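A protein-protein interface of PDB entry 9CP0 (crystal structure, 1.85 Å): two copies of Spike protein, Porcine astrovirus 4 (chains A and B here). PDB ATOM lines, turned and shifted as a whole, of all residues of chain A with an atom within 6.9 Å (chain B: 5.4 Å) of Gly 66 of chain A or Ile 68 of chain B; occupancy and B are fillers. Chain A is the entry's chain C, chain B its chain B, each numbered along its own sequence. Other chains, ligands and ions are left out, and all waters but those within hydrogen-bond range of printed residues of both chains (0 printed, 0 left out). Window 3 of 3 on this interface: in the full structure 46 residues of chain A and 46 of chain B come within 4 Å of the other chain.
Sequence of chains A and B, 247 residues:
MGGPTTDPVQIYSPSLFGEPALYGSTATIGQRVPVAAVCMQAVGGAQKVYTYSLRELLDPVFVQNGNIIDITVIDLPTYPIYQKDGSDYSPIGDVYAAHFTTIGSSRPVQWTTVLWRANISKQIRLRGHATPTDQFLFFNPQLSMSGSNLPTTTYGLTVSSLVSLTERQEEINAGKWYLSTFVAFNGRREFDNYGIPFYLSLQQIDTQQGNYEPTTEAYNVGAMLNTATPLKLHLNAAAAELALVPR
Gly 66 of chain A touches Ile 68 of chain B, and with the chains exchanged Ile 68 of chain A touches Gly 66 of chain B.
Ile 68 of chain A touches Asn 67 of chain B, but with the chains exchanged Asn 67 of chain A does not touch Ile 68 of chain B (4.04 Å).
Ile 68 of chain A touches its own counterpart, Ile 68 of chain B.
Gln 64 of chain A touches none of the printed residues of chain B.
Asn 65 of chain A touches none of the printed residues of chain B.
Of chain B, only Ile 68 (3.1 Å) comes within 4 Å of Gly 66 of chain A.
Printed residues of chain B within 4 Å of Ile 68 of chain A: Gly 66 (3.2 Å), Asn 67 (3.9 Å) and Ile 68 (3.6 Å).
Printed residues of chain A within 4 Å of Gly 66 of chain B: Ile 68.
Of the printed residues of chain A, Asn 67 of chain B touches Ile 68 (3.9 Å).
Ile 68 of chain B touches just these residues of chain A: Gly 66 (3.1 Å) and Ile 68 (3.6 Å).
The nearest printed residue of chain B that does not touch Gly 66 of chain A is Val 61 of chain B (5.6 Å).
The nearest printed residue of chain A that does not touch Gly 66 of chain B is Val 61 of chain A (5.7 Å).
Of the 9 printed residues of chain B, 3 touch a printed residue of chain A.
Along chain B the printed residues that touch a printed residue of chain A span positions 66 to 68.
Of the 9 printed residues of chain A, 2 touch a printed residue of chain B.
Among the printed residues, no Asp or Glu carboxylate lies within 4 Å of a Lys or Arg side-chain nitrogen of the other chain.
Ile 68 of chain B touches Gly 66 of chain A (CD1 to O, 3.1 Å).
Ile 68 of chain A touches Gly 66 of chain B.
Ile 68 of chain A touches Asn 67 of chain B (CD1 to CA, 3.9 Å).
Ile 68 of chain A touches Ile 68 of chain B.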
ATOM      1  N   GLN A  10      -3.026  30.080 -13.169  1.00  0.00           N
ATOM      2  CA  GLN A  10      -2.940  30.546 -11.793  1.00  0.00           C
ATOM      3  C   GLN A  10      -1.816  31.568 -11.673  1.00  0.00           C
ATOM      4  O   GLN A  10      -0.703  31.345 -12.164  1.00  0.00           O
ATOM      5  CB  GLN A  10      -2.705  29.371 -10.844  1.00  0.00           C
ATOM      6  CG  GLN A  10      -3.912  28.464 -10.690  1.00  0.00           C
ATOM      7  CD  GLN A  10      -3.687  27.364  -9.674  1.00  0.00           C
ATOM      8  OE1 GLN A  10      -2.544  26.995  -9.383  1.00  0.00           O
ATOM      9  NE2 GLN A  10      -4.779  26.850  -9.104  1.00  0.00           N
ATOM     10  N   VAL A  61       4.430  34.930 -10.747  1.00  0.00           N
ATOM     11  CA  VAL A  61       4.701  33.572 -11.180  1.00  0.00           C
ATOM     12  C   VAL A  61       3.423  33.045 -11.814  1.00  0.00           C
ATOM     13  O   VAL A  61       2.323  33.259 -11.291  1.00  0.00           O
ATOM     14  CB  VAL A  61       5.157  32.672 -10.011  1.00  0.00           C
ATOM     15  CG1 VAL A  61       5.005  31.194 -10.370  1.00  0.00           C
ATOM     16  CG2 VAL A  61       6.583  33.006  -9.592  1.00  0.00           C
ATOM     17  N   PHE A  62       3.565  32.376 -12.951  1.00  0.00           N
ATOM     18  CA  PHE A  62       2.445  31.893 -13.745  1.00  0.00           C
ATOM     19  C   PHE A  62       2.445  30.372 -13.719  1.00  0.00           C
ATOM     20  O   PHE A  62       3.485  29.749 -13.955  1.00  0.00           O
ATOM     21  CB  PHE A  62       2.559  32.395 -15.183  1.00  0.00           C
ATOM     22  CG  PHE A  62       2.486  33.882 -15.307  1.00  0.00           C
ATOM     23  CD1 PHE A  62       1.382  34.570 -14.847  1.00  0.00           C
ATOM     24  CD2 PHE A  62       3.519  34.592 -15.895  1.00  0.00           C
ATOM     25  CE1 PHE A  62       1.309  35.940 -14.960  1.00  0.00           C
ATOM     26  CE2 PHE A  62       3.453  35.962 -16.013  1.00  0.00           C
ATOM     27  CZ  PHE A  62       2.346  36.642 -15.540  1.00  0.00           C
ATOM     28  N   VAL A  63       1.285  29.777 -13.452  1.00  0.00           N
ATOM     29  CA  VAL A  63       1.172  28.330 -13.316  1.00  0.00           C
ATOM     30  C   VAL A  63      -0.013  27.850 -14.140  1.00  0.00           C
ATOM     31  O   VAL A  63      -1.116  28.387 -14.014  1.00  0.00           O
ATOM     32  CB  VAL A  63       1.016  27.905 -11.843  1.00  0.00           C
ATOM     33  CG1 VAL A  63       0.660  26.428 -11.751  1.00  0.00           C
ATOM     34  CG2 VAL A  63       2.280  28.220 -11.060  1.00  0.00           C
ATOM     35  N   GLN A  64       0.210  26.839 -14.979  1.00  0.00           N
ATOM     36  CA  GLN A  64      -0.856  26.223 -15.759  1.00  0.00           C
ATOM     37  C   GLN A  64      -0.818  24.719 -15.543  1.00  0.00           C
ATOM     38  O   GLN A  64       0.210  24.078 -15.790  1.00  0.00           O
ATOM     39  CB  GLN A  64      -0.724  26.552 -17.248  1.00  0.00           C
ATOM     40  CG  GLN A  64      -2.011  26.347 -18.040  1.00  0.00           C
ATOM     41  CD  GLN A  64      -1.769  26.284 -19.537  1.00  0.00           C
ATOM     42  OE1 GLN A  64      -0.926  25.517 -20.006  1.00  0.00           O
ATOM     43  NE2 GLN A  64      -2.495  27.102 -20.293  1.00  0.00           N
ATOM     44  N   ASN A  65      -1.941  24.162 -15.083  1.00  0.00           N
ATOM     45  CA  ASN A  65      -2.099  22.718 -14.890  1.00  0.00           C
ATOM     46  C   ASN A  65      -0.998  22.143 -13.997  1.00  0.00           C
ATOM     47  O   ASN A  65      -0.506  21.034 -14.223  1.00  0.00           O
ATOM     48  CB  ASN A  65      -2.150  21.984 -16.232  1.00  0.00           C
ATOM     49  CG  ASN A  65      -3.565  21.830 -16.762  1.00  0.00           C
ATOM     50  OD1 ASN A  65      -4.481  21.452 -16.027  1.00  0.00           O
ATOM     51  ND2 ASN A  65      -3.748  22.116 -18.051  1.00  0.00           N
ATOM     52  N   GLY A  66      -0.609  22.902 -12.975  1.00  0.00           N
ATOM     53  CA  GLY A  66       0.387  22.444 -12.027  1.00  0.00           C
ATOM     54  C   GLY A  66       1.826  22.651 -12.437  1.00  0.00           C
ATOM     55  O   GLY A  66       2.726  22.154 -11.748  1.00  0.00           O
ATOM     56  N   ASN A  67       2.075  23.366 -13.530  1.00  0.00           N
ATOM     57  CA  ASN A  67       3.424  23.604 -14.018  1.00  0.00           C
ATOM     58  C   ASN A  67       3.635  25.097 -14.212  1.00  0.00           C
ATOM     59  O   ASN A  67       2.765  25.786 -14.742  1.00  0.00           O
ATOM     60  CB  ASN A  67       3.662  22.840 -15.330  1.00  0.00           C
ATOM     61  CG  ASN A  67       3.381  21.356 -15.189  1.00  0.00           C
ATOM     62  OD1 ASN A  67       2.683  20.760 -16.011  1.00  0.00           O
ATOM     63  ND2 ASN A  67       3.918  20.753 -14.133  1.00  0.00           N
ATOM     64  N   ILE A  68       4.781  25.591 -13.743  1.00  0.00           N
ATOM     65  CA  ILE A  68       5.177  26.977 -13.975  1.00  0.00           C
ATOM     66  C   ILE A  68       5.482  27.163 -15.456  1.00  0.00           C
ATOM     67  O   ILE A  68       6.226  26.378 -16.055  1.00  0.00           O
ATOM     68  CB  ILE A  68       6.394  27.332 -13.105  1.00  0.00           C
ATOM     69  CG1 ILE A  68       6.018  27.344 -11.615  1.00  0.00           C
ATOM     70  CG2 ILE A  68       7.015  28.655 -13.521  1.00  0.00           C
ATOM     71  CD1 ILE A  68       7.202  27.550 -10.699  1.00  0.00           C
ATOM     72  N   VAL B  61       0.302  24.467  -3.617  1.00  0.00           N
ATOM     73  CA  VAL B  61       1.470  24.395  -4.481  1.00  0.00           C
ATOM     74  C   VAL B  61       2.615  25.053  -3.730  1.00  0.00           C
ATOM     75  O   VAL B  61       2.449  26.133  -3.157  1.00  0.00           O
ATOM     76  CB  VAL B  61       1.226  25.076  -5.845  1.00  0.00           C
ATOM     77  CG1 VAL B  61       2.537  25.467  -6.494  1.00  0.00           C
ATOM     78  CG2 VAL B  61       0.423  24.158  -6.747  1.00  0.00           C
ATOM     79  N   PHE B  62       3.757  24.383  -3.687  1.00  0.00           N
ATOM     80  CA  PHE B  62       4.919  24.890  -2.982  1.00  0.00           C
ATOM     81  C   PHE B  62       5.960  25.309  -4.007  1.00  0.00           C
ATOM     82  O   PHE B  62       6.271  24.546  -4.924  1.00  0.00           O
ATOM     83  CB  PHE B  62       5.490  23.836  -2.034  1.00  0.00           C
ATOM     84  CG  PHE B  62       4.479  23.262  -1.086  1.00  0.00           C
ATOM     85  CD1 PHE B  62       3.830  24.075  -0.172  1.00  0.00           C
ATOM     86  CD2 PHE B  62       4.134  21.921  -1.147  1.00  0.00           C
ATOM     87  CE1 PHE B  62       2.882  23.553   0.691  1.00  0.00           C
ATOM     88  CE2 PHE B  62       3.196  21.393  -0.286  1.00  0.00           C
ATOM     89  CZ  PHE B  62       2.564  22.213   0.637  1.00  0.00           C
ATOM     90  N   VAL B  63       6.492  26.518  -3.852  1.00  0.00           N
ATOM     91  CA  VAL B  63       7.477  27.062  -4.774  1.00  0.00           C
ATOM     92  C   VAL B  63       8.679  27.514  -3.970  1.00  0.00           C
ATOM     93  O   VAL B  63       8.540  28.270  -3.003  1.00  0.00           O
ATOM     94  CB  VAL B  63       6.915  28.230  -5.603  1.00  0.00           C
ATOM     95  CG1 VAL B  63       8.051  28.994  -6.269  1.00  0.00           C
ATOM     96  CG2 VAL B  63       5.921  27.715  -6.632  1.00  0.00           C
ATOM     97  N   GLN B  64       9.855  27.055  -4.373  1.00  0.00           N
ATOM     98  CA  GLN B  64      11.092  27.401  -3.694  1.00  0.00           C
ATOM     99  C   GLN B  64      12.074  27.919  -4.734  1.00  0.00           C
ATOM    100  O   GLN B  64      12.424  27.201  -5.680  1.00  0.00           O
ATOM    101  CB  GLN B  64      11.661  26.198  -2.939  1.00  0.00           C
ATOM    102  CG  GLN B  64      12.933  26.503  -2.172  1.00  0.00           C
ATOM    103  CD  GLN B  64      13.544  25.263  -1.556  1.00  0.00           C
ATOM    104  OE1 GLN B  64      13.284  24.948  -0.392  1.00  0.00           O
ATOM    105  NE2 GLN B  64      14.353  24.547  -2.332  1.00  0.00           N
ATOM    106  N   GLY B  66      11.762  29.786  -7.168  1.00  0.00           N
ATOM    107  CA  GLY B  66      11.241  29.850  -8.515  1.00  0.00           C
ATOM    108  C   GLY B  66      10.712  28.553  -9.088  1.00  0.00           C
ATOM    109  O   GLY B  66      10.191  28.568 -10.210  1.00  0.00           O
ATOM    110  N   ASN B  67      10.816  27.438  -8.367  1.00  0.00           N
ATOM    111  CA  ASN B  67      10.413  26.148  -8.909  1.00  0.00           C
ATOM    112  C   ASN B  67       9.494  25.413  -7.948  1.00  0.00           C
ATOM    113  O   ASN B  67       9.737  25.383  -6.739  1.00  0.00           O
ATOM    114  CB  ASN B  67      11.639  25.281  -9.226  1.00  0.00           C
ATOM    115  CG  ASN B  67      12.652  26.007 -10.082  1.00  0.00           C
ATOM    116  OD1 ASN B  67      12.308  26.599 -11.114  1.00  0.00           O
ATOM    117  ND2 ASN B  67      13.910  25.981  -9.655  1.00  0.00           N
ATOM    118  N   ILE B  68       8.436  24.820  -8.508  1.00  0.00           N
ATOM    119  CA  ILE B  68       7.560  23.939  -7.746  1.00  0.00           C
ATOM    120  C   ILE B  68       8.371  22.785  -7.174  1.00  0.00           C
ATOM    121  O   ILE B  68       9.187  22.175  -7.873  1.00  0.00           O
ATOM    122  CB  ILE B  68       6.428  23.428  -8.653  1.00  0.00           C
ATOM    123  CG1 ILE B  68       5.651  24.606  -9.243  1.00  0.00           C
ATOM    124  CG2 ILE B  68       5.508  22.483  -7.897  1.00  0.00           C
ATOM    125  CD1 ILE B  68       4.538  24.193 -10.178  1.00  0.00           C
ATOM    126  N   ILE B  69       8.167  22.485  -5.884  1.00  0.00           N
ATOM    127  CA  ILE B  69       8.885  21.392  -5.240  1.00  0.00           C
ATOM    128  C   ILE B  69       7.915  20.479  -4.499  1.00  0.00           C
ATOM    129  O   ILE B  69       6.790  20.859  -4.163  1.00  0.00           O
ATOM    130  CB  ILE B  69      10.013  21.913  -4.293  1.00  0.00           C
ATOM    131  CG1 ILE B  69       9.541  22.810  -3.131  1.00  0.00           C
ATOM    132  CG2 ILE B  69      11.069  22.655  -5.089  1.00  0.00           C
ATOM    133  CD1 ILE B  69       8.588  22.233  -2.098  1.00  0.00           C
ATOM    134  N   ASP B  70       8.371  19.249  -4.257  1.00  0.00           N
ATOM    135  CA  ASP B  70       7.658  18.280  -3.434  1.00  0.00           C
ATOM    136  C   ASP B  70       8.276  18.343  -2.042  1.00  0.00           C
ATOM    137  O   ASP B  70       9.309  17.728  -1.783  1.00  0.00           O
ATOM    138  CB  ASP B  70       7.758  16.876  -4.016  1.00  0.00           C
ATOM    139  CG  ASP B  70       6.594  15.998  -3.611  1.00  0.00           C
ATOM    140  OD1 ASP B  70       6.303  15.917  -2.398  1.00  0.00           O
ATOM    141  OD2 ASP B  70       5.998  15.356  -4.501  1.00  0.00           O
